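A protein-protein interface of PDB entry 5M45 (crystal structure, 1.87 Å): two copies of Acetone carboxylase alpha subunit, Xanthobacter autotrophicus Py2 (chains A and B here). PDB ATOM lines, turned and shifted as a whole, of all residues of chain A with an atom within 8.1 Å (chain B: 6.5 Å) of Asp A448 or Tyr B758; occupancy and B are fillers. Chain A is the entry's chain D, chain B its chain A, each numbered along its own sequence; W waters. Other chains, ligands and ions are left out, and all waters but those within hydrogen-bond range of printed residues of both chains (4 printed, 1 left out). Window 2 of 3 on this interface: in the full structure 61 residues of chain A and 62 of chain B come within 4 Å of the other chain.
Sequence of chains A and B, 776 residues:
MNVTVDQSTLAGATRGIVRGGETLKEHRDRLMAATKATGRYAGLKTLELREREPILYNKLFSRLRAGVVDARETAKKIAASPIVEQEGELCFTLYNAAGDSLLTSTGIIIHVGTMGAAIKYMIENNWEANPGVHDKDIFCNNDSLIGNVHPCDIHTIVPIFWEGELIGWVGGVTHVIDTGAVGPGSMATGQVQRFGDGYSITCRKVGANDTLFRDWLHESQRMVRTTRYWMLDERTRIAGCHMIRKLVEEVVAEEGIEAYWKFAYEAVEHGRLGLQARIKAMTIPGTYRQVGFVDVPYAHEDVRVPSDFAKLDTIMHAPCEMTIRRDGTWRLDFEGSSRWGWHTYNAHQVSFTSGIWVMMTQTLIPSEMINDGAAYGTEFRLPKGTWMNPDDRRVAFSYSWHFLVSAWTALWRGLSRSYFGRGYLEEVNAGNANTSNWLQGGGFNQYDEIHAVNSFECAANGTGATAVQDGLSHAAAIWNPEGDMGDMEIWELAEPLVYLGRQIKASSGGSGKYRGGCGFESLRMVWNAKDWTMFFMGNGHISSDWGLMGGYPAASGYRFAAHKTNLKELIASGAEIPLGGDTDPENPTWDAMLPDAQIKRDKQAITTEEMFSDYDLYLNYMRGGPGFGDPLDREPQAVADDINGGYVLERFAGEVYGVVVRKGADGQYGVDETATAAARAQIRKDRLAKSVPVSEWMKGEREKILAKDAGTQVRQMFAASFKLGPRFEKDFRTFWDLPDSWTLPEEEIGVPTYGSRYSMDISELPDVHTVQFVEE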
ATOM      1  N   GLY A 443      21.886  19.536   3.383  1.00  0.00           N
ATOM      2  CA  GLY A 443      21.769  20.180   4.711  1.00  0.00           C
ATOM      3  C   GLY A 443      20.435  19.840   5.343  1.00  0.00           C
ATOM      4  O   GLY A 443      19.930  18.702   5.168  1.00  0.00           O
ATOM      5  N   PHE A 444      19.858  20.775   6.084  1.00  0.00           N
ATOM      6  CA  PHE A 444      18.519  20.575   6.702  1.00  0.00           C
ATOM      7  C   PHE A 444      17.383  21.138   5.847  1.00  0.00           C
ATOM      8  O   PHE A 444      17.452  22.269   5.368  1.00  0.00           O
ATOM      9  CB  PHE A 444      18.449  21.149   8.147  1.00  0.00           C
ATOM     10  CG  PHE A 444      18.958  20.192   9.184  1.00  0.00           C
ATOM     11  CD1 PHE A 444      20.274  19.923   9.291  1.00  0.00           C
ATOM     12  CD2 PHE A 444      18.083  19.522  10.031  1.00  0.00           C
ATOM     13  CE1 PHE A 444      20.756  18.998  10.238  1.00  0.00           C
ATOM     14  CE2 PHE A 444      18.563  18.589  10.964  1.00  0.00           C
ATOM     15  CZ  PHE A 444      19.891  18.320  11.046  1.00  0.00           C
ATOM     16  N   ASN A 445      16.319  20.353   5.712  1.00  0.00           N
ATOM     17  CA  ASN A 445      15.168  20.742   4.896  1.00  0.00           C
ATOM     18  C   ASN A 445      14.017  21.362   5.723  1.00  0.00           C
ATOM     19  O   ASN A 445      14.158  21.681   6.933  1.00  0.00           O
ATOM     20  CB  ASN A 445      14.725  19.548   4.035  1.00  0.00           C
ATOM     21  CG  ASN A 445      14.109  18.447   4.826  1.00  0.00           C
ATOM     22  OD1 ASN A 445      13.839  18.572   6.051  1.00  0.00           O
ATOM     23  ND2 ASN A 445      13.895  17.313   4.158  1.00  0.00           N
ATOM     24  N   GLN A 446      12.874  21.548   5.067  1.00  0.00           N
ATOM     25  CA  GLN A 446      11.686  22.148   5.718  1.00  0.00           C
ATOM     26  C   GLN A 446      11.063  21.281   6.812  1.00  0.00           C
ATOM     27  O   GLN A 446      10.242  21.763   7.568  1.00  0.00           O
ATOM     28  CB  GLN A 446      10.629  22.544   4.665  1.00  0.00           C
ATOM     29  CG  GLN A 446      10.077  21.419   3.784  1.00  0.00           C
ATOM     30  CD  GLN A 446      10.793  21.251   2.458  1.00  0.00           C
ATOM     31  OE1 GLN A 446      12.017  21.155   2.401  1.00  0.00           O
ATOM     32  NE2 GLN A 446      10.019  21.195   1.368  1.00  0.00           N
ATOM     33  N   TYR A 447      11.401  19.984   6.841  1.00  0.00           N
ATOM     34  CA  TYR A 447      10.923  19.060   7.870  1.00  0.00           C
ATOM     35  C   TYR A 447      11.969  18.900   8.993  1.00  0.00           C
ATOM     36  O   TYR A 447      11.822  18.000   9.833  1.00  0.00           O
ATOM     37  CB  TYR A 447      10.579  17.688   7.251  1.00  0.00           C
ATOM     38  CG  TYR A 447       9.747  17.793   5.957  1.00  0.00           C
ATOM     39  CD1 TYR A 447       8.428  18.270   5.990  1.00  0.00           C
ATOM     40  CD2 TYR A 447      10.294  17.445   4.700  1.00  0.00           C
ATOM     41  CE1 TYR A 447       7.670  18.379   4.845  1.00  0.00           C
ATOM     42  CE2 TYR A 447       9.550  17.573   3.535  1.00  0.00           C
ATOM     43  CZ  TYR A 447       8.212  18.057   3.606  1.00  0.00           C
ATOM     44  OH  TYR A 447       7.443  18.227   2.443  1.00  0.00           O
ATOM     45  N   ASP A 448      13.012  19.738   9.012  1.00  0.00           N
ATOM     46  CA  ASP A 448      14.080  19.664  10.035  1.00  0.00           C
ATOM     47  C   ASP A 448      14.788  18.300  10.108  1.00  0.00           C
ATOM     48  O   ASP A 448      15.081  17.814  11.171  1.00  0.00           O
ATOM     49  CB  ASP A 448      13.546  20.127  11.404  1.00  0.00           C
ATOM     50  CG  ASP A 448      13.037  21.596  11.377  1.00  0.00           C
ATOM     51  OD1 ASP A 448      13.586  22.462  10.663  1.00  0.00           O
ATOM     52  OD2 ASP A 448      12.069  21.931  12.080  1.00  0.00           O
ATOM     53  N   GLU A 449      15.087  17.725   8.953  1.00  0.00           N
ATOM     54  CA  GLU A 449      15.819  16.470   8.805  1.00  0.00           C
ATOM     55  C   GLU A 449      17.001  16.661   7.858  1.00  0.00           C
ATOM     56  O   GLU A 449      16.996  17.545   6.988  1.00  0.00           O
ATOM     57  CB  GLU A 449      14.918  15.387   8.199  1.00  0.00           C
ATOM     58  CG  GLU A 449      13.871  14.924   9.223  1.00  0.00           C
ATOM     59  CD  GLU A 449      12.942  13.813   8.696  1.00  0.00           C
ATOM     60  OE1 GLU A 449      12.143  13.299   9.531  1.00  0.00           O
ATOM     61  OE2 GLU A 449      13.009  13.456   7.475  1.00  0.00           O
ATOM     62  N   ILE A 450      17.989  15.789   8.005  1.00  0.00           N
ATOM     63  CA  ILE A 450      19.106  15.737   7.085  1.00  0.00           C
ATOM     64  C   ILE A 450      18.560  15.362   5.704  1.00  0.00           C
ATOM     65  O   ILE A 450      17.711  14.458   5.584  1.00  0.00           O
ATOM     66  CB  ILE A 450      20.175  14.748   7.585  1.00  0.00           C
ATOM     67  CG1 ILE A 450      20.845  15.263   8.849  1.00  0.00           C
ATOM     68  CG2 ILE A 450      21.210  14.468   6.494  1.00  0.00           C
ATOM     69  CD1 ILE A 450      21.703  14.237   9.584  1.00  0.00           C
ATOM     70  N   HIS A 451      19.064  16.037   4.672  1.00  0.00           N
ATOM     71  CA  HIS A 451      18.522  15.928   3.316  1.00  0.00           C
ATOM     72  C   HIS A 451      19.537  16.252   2.216  1.00  0.00           C
ATOM     73  O   HIS A 451      20.605  16.859   2.455  1.00  0.00           O
ATOM     74  CB  HIS A 451      17.316  16.864   3.229  1.00  0.00           C
ATOM     75  CG  HIS A 451      16.413  16.654   2.039  1.00  0.00           C
ATOM     76  ND1 HIS A 451      15.763  15.471   1.794  1.00  0.00           N
ATOM     77  CD2 HIS A 451      15.980  17.525   1.093  1.00  0.00           C
ATOM     78  CE1 HIS A 451      15.022  15.604   0.708  1.00  0.00           C
ATOM     79  NE2 HIS A 451      15.118  16.852   0.280  1.00  0.00           N
ATOM     80  N   ASN A 528      13.079  28.027   3.852  1.00  0.00           N
ATOM     81  CA  ASN A 528      12.886  27.059   4.941  1.00  0.00           C
ATOM     82  C   ASN A 528      14.004  25.979   4.968  1.00  0.00           C
ATOM     83  O   ASN A 528      13.763  24.827   5.400  1.00  0.00           O
ATOM     84  CB  ASN A 528      11.479  26.436   4.861  1.00  0.00           C
ATOM     85  CG  ASN A 528      10.887  26.081   6.216  1.00  0.00           C
ATOM     86  OD1 ASN A 528      11.511  26.279   7.280  1.00  0.00           O
ATOM     87  ND2 ASN A 528       9.656  25.579   6.193  1.00  0.00           N
ATOM     88  N   ALA A 529      15.204  26.334   4.465  1.00  0.00           N
ATOM     89  CA  ALA A 529      16.407  25.505   4.578  1.00  0.00           C
ATOM     90  C   ALA A 529      17.273  26.004   5.769  1.00  0.00           C
ATOM     91  O   ALA A 529      17.285  27.205   6.094  1.00  0.00           O
ATOM     92  CB  ALA A 529      17.230  25.593   3.297  1.00  0.00           C
ATOM     93  N   LYS A 530      18.050  25.090   6.354  1.00  0.00           N
ATOM     94  CA  LYS A 530      19.037  25.438   7.384  1.00  0.00           C
ATOM     95  C   LYS A 530      20.367  24.730   7.092  1.00  0.00           C
ATOM     96  O   LYS A 530      20.380  23.586   6.618  1.00  0.00           O
ATOM     97  CB  LYS A 530      18.542  25.068   8.783  1.00  0.00           C
ATOM     98  CG  LYS A 530      17.166  25.664   9.129  1.00  0.00           C
ATOM     99  CD  LYS A 530      16.029  24.708   8.781  1.00  0.00           C
ATOM    100  CE  LYS A 530      14.680  25.418   8.733  1.00  0.00           C
ATOM    101  NZ  LYS A 530      13.579  24.515   8.345  1.00  0.00           N
ATOM    102  N   ASP A 531      21.473  25.417   7.380  1.00  0.00           N
ATOM    103  CA  ASP A 531      22.805  24.842   7.196  1.00  0.00           C
ATOM    104  C   ASP A 531      22.952  24.212   5.807  1.00  0.00           C
ATOM    105  O   ASP A 531      23.334  23.047   5.657  1.00  0.00           O
ATOM    106  CB  ASP A 531      23.095  23.836   8.333  1.00  0.00           C
ATOM    107  CG  ASP A 531      23.167  24.489   9.718  1.00  0.00           C
ATOM    108  OD1 ASP A 531      23.206  25.743   9.827  1.00  0.00           O
ATOM    109  OD2 ASP A 531      23.251  23.712  10.722  1.00  0.00           O
ATOM    110  N   TRP B 340      31.142  18.735  18.815  1.00  0.00           N
ATOM    111  CA  TRP B 340      31.639  18.048  17.602  1.00  0.00           C
ATOM    112  C   TRP B 340      31.900  19.055  16.472  1.00  0.00           C
ATOM    113  O   TRP B 340      31.395  20.186  16.508  1.00  0.00           O
ATOM    114  CB  TRP B 340      30.659  16.942  17.160  1.00  0.00           C
ATOM    115  CG  TRP B 340      29.283  17.443  16.777  1.00  0.00           C
ATOM    116  CD1 TRP B 340      28.201  17.547  17.599  1.00  0.00           C
ATOM    117  CD2 TRP B 340      28.846  17.854  15.486  1.00  0.00           C
ATOM    118  NE1 TRP B 340      27.122  18.032  16.904  1.00  0.00           N
ATOM    119  CE2 TRP B 340      27.486  18.232  15.603  1.00  0.00           C
ATOM    120  CE3 TRP B 340      29.467  17.963  14.250  1.00  0.00           C
ATOM    121  CZ2 TRP B 340      26.721  18.676  14.516  1.00  0.00           C
ATOM    122  CZ3 TRP B 340      28.693  18.430  13.161  1.00  0.00           C
ATOM    123  CH2 TRP B 340      27.340  18.760  13.306  1.00  0.00           C
ATOM    124  N   ASP B 392      24.872  13.975  16.266  1.00  0.00           N
ATOM    125  CA  ASP B 392      24.647  14.067  14.815  1.00  0.00           C
ATOM    126  C   ASP B 392      25.278  12.896  14.078  1.00  0.00           C
ATOM    127  O   ASP B 392      26.469  12.643  14.211  1.00  0.00           O
ATOM    128  CB  ASP B 392      25.155  15.393  14.226  1.00  0.00           C
ATOM    129  CG  ASP B 392      24.646  15.632  12.813  1.00  0.00           C
ATOM    130  OD1 ASP B 392      25.175  15.038  11.839  1.00  0.00           O
ATOM    131  OD2 ASP B 392      23.649  16.381  12.654  1.00  0.00           O
ATOM    132  N   ARG B 394      26.177  12.471  11.098  1.00  0.00           N
ATOM    133  CA  ARG B 394      27.117  12.769   9.996  1.00  0.00           C
ATOM    134  C   ARG B 394      28.582  12.898  10.386  1.00  0.00           C
ATOM    135  O   ARG B 394      29.401  13.082   9.494  1.00  0.00           O
ATOM    136  CB  ARG B 394      26.710  14.057   9.249  1.00  0.00           C
ATOM    137  CG  ARG B 394      25.363  13.939   8.540  1.00  0.00           C
ATOM    138  CD  ARG B 394      24.843  15.287   8.060  1.00  0.00           C
ATOM    139  NE  ARG B 394      24.592  16.141   9.190  1.00  0.00           N
ATOM    140  CZ  ARG B 394      24.324  17.437   9.129  1.00  0.00           C
ATOM    141  NH1 ARG B 394      24.266  18.080   7.961  1.00  0.00           N
ATOM    142  NH2 ARG B 394      24.141  18.107  10.249  1.00  0.00           N
ATOM    143  N   TYR B 754      27.579  25.937  11.001  1.00  0.00           N
ATOM    144  CA  TYR B 754      26.738  24.777  10.631  1.00  0.00           C
ATOM    145  C   TYR B 754      26.870  23.689  11.679  1.00  0.00           C
ATOM    146  O   TYR B 754      27.977  23.353  12.139  1.00  0.00           O
ATOM    147  CB  TYR B 754      27.090  24.239   9.227  1.00  0.00           C
ATOM    148  CG  TYR B 754      26.558  25.052   8.031  1.00  0.00           C
ATOM    149  CD1 TYR B 754      26.252  26.402   8.140  1.00  0.00           C
ATOM    150  CD2 TYR B 754      26.425  24.452   6.770  1.00  0.00           C
ATOM    151  CE1 TYR B 754      25.781  27.123   7.048  1.00  0.00           C
ATOM    152  CE2 TYR B 754      25.955  25.171   5.672  1.00  0.00           C
ATOM    153  CZ  TYR B 754      25.671  26.520   5.803  1.00  0.00           C
ATOM    154  OH  TYR B 754      25.177  27.251   4.768  1.00  0.00           O
ATOM    155  N   GLY B 755      25.736  23.160  12.094  1.00  0.00           N
ATOM    156  CA  GLY B 755      25.646  22.178  13.138  1.00  0.00           C
ATOM    157  C   GLY B 755      25.557  22.694  14.569  1.00  0.00           C
ATOM    158  O   GLY B 755      25.421  21.872  15.497  1.00  0.00           O
ATOM    159  N   SER B 756      25.598  23.996  14.790  1.00  0.00           N
ATOM    160  CA  SER B 756      25.510  24.533  16.156  1.00  0.00           C
ATOM    161  C   SER B 756      24.118  24.425  16.783  1.00  0.00           C
ATOM    162  O   SER B 756      23.994  24.371  18.022  1.00  0.00           O
ATOM    163  CB  SER B 756      25.971  25.991  16.214  1.00  0.00           C
ATOM    164  OG  SER B 756      25.079  26.823  15.549  1.00  0.00           O
ATOM    165  N   ARG B 757      23.076  24.411  15.953  1.00  0.00           N
ATOM    166  CA  ARG B 757      21.684  24.382  16.413  1.00  0.00           C
ATOM    167  C   ARG B 757      20.920  23.184  15.843  1.00  0.00           C
ATOM    168  O   ARG B 757      20.140  22.550  16.562  1.00  0.00           O
ATOM    169  CB  ARG B 757      20.987  25.689  16.064  1.00  0.00           C
ATOM    170  CG  ARG B 757      21.545  26.886  16.843  1.00  0.00           C
ATOM    171  CD  ARG B 757      20.982  28.245  16.497  1.00  0.00           C
ATOM    172  NE  ARG B 757      20.041  28.762  17.528  1.00  0.00           N
ATOM    173  CZ  ARG B 757      20.347  29.188  18.770  1.00  0.00           C
ATOM    174  NH1 ARG B 757      21.612  29.193  19.237  1.00  0.00           N
ATOM    175  NH2 ARG B 757      19.352  29.599  19.568  1.00  0.00           N
ATOM    176  N   TYR B 758      21.128  22.847  14.576  1.00  0.00           N
ATOM    177  CA  TYR B 758      20.442  21.730  13.939  1.00  0.00           C
ATOM    178  C   TYR B 758      21.317  20.483  13.916  1.00  0.00           C
ATOM    179  O   TYR B 758      22.434  20.512  13.387  1.00  0.00           O
ATOM    180  CB  TYR B 758      19.991  22.126  12.536  1.00  0.00           C
ATOM    181  CG  TYR B 758      18.909  23.171  12.579  1.00  0.00           C
ATOM    182  CD1 TYR B 758      19.217  24.545  12.651  1.00  0.00           C
ATOM    183  CD2 TYR B 758      17.557  22.794  12.643  1.00  0.00           C
ATOM    184  CE1 TYR B 758      18.203  25.500  12.755  1.00  0.00           C
ATOM    185  CE2 TYR B 758      16.566  23.736  12.743  1.00  0.00           C
ATOM    186  CZ  TYR B 758      16.895  25.084  12.788  1.00  0.00           C
ATOM    187  OH  TYR B 758      15.852  25.971  12.824  1.00  0.00           O
ATOM    188  N   SER B 759      20.796  19.394  14.497  1.00  0.00           N
ATOM    189  CA  SER B 759      21.499  18.105  14.528  1.00  0.00           C
ATOM    190  C   SER B 759      20.477  16.938  14.534  1.00  0.00           C
ATOM    191  O   SER B 759      19.353  17.107  14.989  1.00  0.00           O
ATOM    192  CB  SER B 759      22.423  18.050  15.749  1.00  0.00           C
ATOM    193  OG  SER B 759      21.649  18.251  16.917  1.00  0.00           O
ATOM    194  N   MET B 760      20.862  15.793  13.994  1.00  0.00           N
ATOM    195  CA  MET B 760      19.997  14.612  13.933  1.00  0.00           C
ATOM    196  C   MET B 760      20.790  13.387  14.390  1.00  0.00           C
ATOM    197  O   MET B 760      21.722  12.946  13.710  1.00  0.00           O
ATOM    198  CB  MET B 760      19.472  14.437  12.504  1.00  0.00           C
ATOM    199  CG  MET B 760      18.443  13.341  12.302  1.00  0.00           C
ATOM    200  SD  MET B 760      18.127  12.935  10.521  1.00  0.00           S
ATOM    201  CE  MET B 760      16.614  11.987  10.713  1.00  0.00           C
ATOM    202  N   GLU B 764      17.337   8.593  15.902  1.00  0.00           N
ATOM    203  CA  GLU B 764      16.167   9.069  15.173  1.00  0.00           C
ATOM    204  C   GLU B 764      15.849   8.235  13.918  1.00  0.00           C
ATOM    205  O   GLU B 764      14.786   8.391  13.359  1.00  0.00           O
ATOM    206  CB  GLU B 764      16.300  10.578  14.816  1.00  0.00           C
ATOM    207  CG  GLU B 764      16.418  11.438  16.089  1.00  0.00           C
ATOM    208  CD  GLU B 764      16.743  12.893  15.836  1.00  0.00           C
ATOM    209  OE1 GLU B 764      16.019  13.462  14.991  1.00  0.00           O
ATOM    210  OE2 GLU B 764      17.715  13.469  16.451  1.00  0.00           O
HETATM  211  O   HOH W   1      17.355  12.269   7.424  1.00  0.00           O
HETATM  212  O   HOH W   2      23.474  21.205  10.327  1.00  0.00           O
HETATM  213  O   HOH W   3      13.402  24.959  12.157  1.00  0.00           O
HETATM  214  O   HOH W   4      23.996  20.839   7.343  1.00  0.00           O
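The backbone NH (N) of Gly B755 sits at hydrogen-bond distance from the side-chain carboxylate (OD2) of Asp A531 (2.9 Å).
N of Met B760 lies within hydrogen-bond range of OD2 of Asp B392 (3.1 Å).
N of Asp A448 is in hydrogen-bond range of OD1 of Asn A445 (3.3 Å).
The backbone carbonyl oxygen (O) of Lys A530 is in hydrogen-bond range of the backbone NH (N) of Phe A444, 2.9 Å away.
The side-chain amide oxygen (OD1) of Asn A528 sits at hydrogen-bond distance from the side-chain amino group (NZ) of Lys A530 (2.9 Å).
The side-chain carboxylate (OD1) of Asp B392 lies within salt-bridge range of the guanidinium group (NE) of Arg B394, at 2.9 Å.
OD1 of Asp A448 is in salt-bridge range of NZ of Lys A530, at 3.1 Å.
Phe A444 touches Arg B394 (CE1 to NH2, 3.5 Å).
Phe A444 touches Tyr B758 (CZ to C, 3.9 Å).
Phe A444 touches Ser B759.
CE2 of Tyr B758 touches OD1 of Asp A448, at 3.9 Å.
Ile A450 touches Arg B394 (CD1 to NE, 3.5 Å).
CD1 of Ile A450 touches CB of Met B760, 3.7 Å away.
Tyr B758 touches Lys A530.
Tyr B754 touches Asp A531 (CE2 to C, 3.2 Å).
Printed residues of chain B within 4 Å of Phe A444: Arg B394 (3.5 Å), Tyr B758 (3.9 Å) and Ser B759 (3.7 Å).
Tyr A447 touches none of the printed residues of chain B.
Asp A448 touches just one residue of chain B: Tyr B758 (3.9 Å).
Printed residues of chain B within 4 Å of Asp A531: Tyr B754 (3.2 Å) and Gly B755 (2.9 Å).
Ser B756 touches none of the printed residues of chain A.
Of chain A, only Phe A444 (3.9 Å), Asp A448 (3.9 Å) and Lys A530 (3.7 Å) come within 4 Å of Tyr B758.
Of the printed residues of chain A, Met B760 touches Ile A450 (3.7 Å).
The nearest printed residue of chain B that does not touch Asp A531 is Tyr B758 (4.1 Å).
Hydrophobic or aromatic side chains of chain A that line the printed part of chain B: Phe A444 and Ile A450.
Printed residues of chain B that touch a printed residue of chain A: Arg B394, Tyr B754, Gly B755, Tyr B758, Ser B759 and Met B760.
Hydrophobic or aromatic side chains of chain B that line the printed part of chain A: Tyr B754, Tyr B758 and Met B760.
Along chain B the printed residues that touch a printed residue of chain A span positions 394 to 760.
Among the printed residues, no Asp or Glu carboxylate lies within 4 Å of a Lys or Arg side-chain nitrogen of the other chain.
No position is printed for both chains.
Of the 9 pairs that touch across the chains among the printed residues, none has its exchanged pair printed and touching as well.
Water W2 lies within hydrogen-bond range of the side-chain carboxylate (OD2) of Asp A531 (2.5 Å), the guanidinium group (NH2) of Arg B394 (3.2 Å), the backbone carbonyl oxygen (O) of Tyr B758 (3.3 Å) and the backbone NH (N) of Gly B755 (3.5 Å).
Water W3 bridges the side-chain hydroxyl of Tyr B758 and the side-chain carboxylate of Asp A448.
Water W4 bridges NH1 of Arg B394 (2.8 Å) and O of Asp A531 (2.9 Å).
Water W1 lies within hydrogen-bond range of O of Ile A450 (2.9 Å) and SD of Met B760 (3.3 Å).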
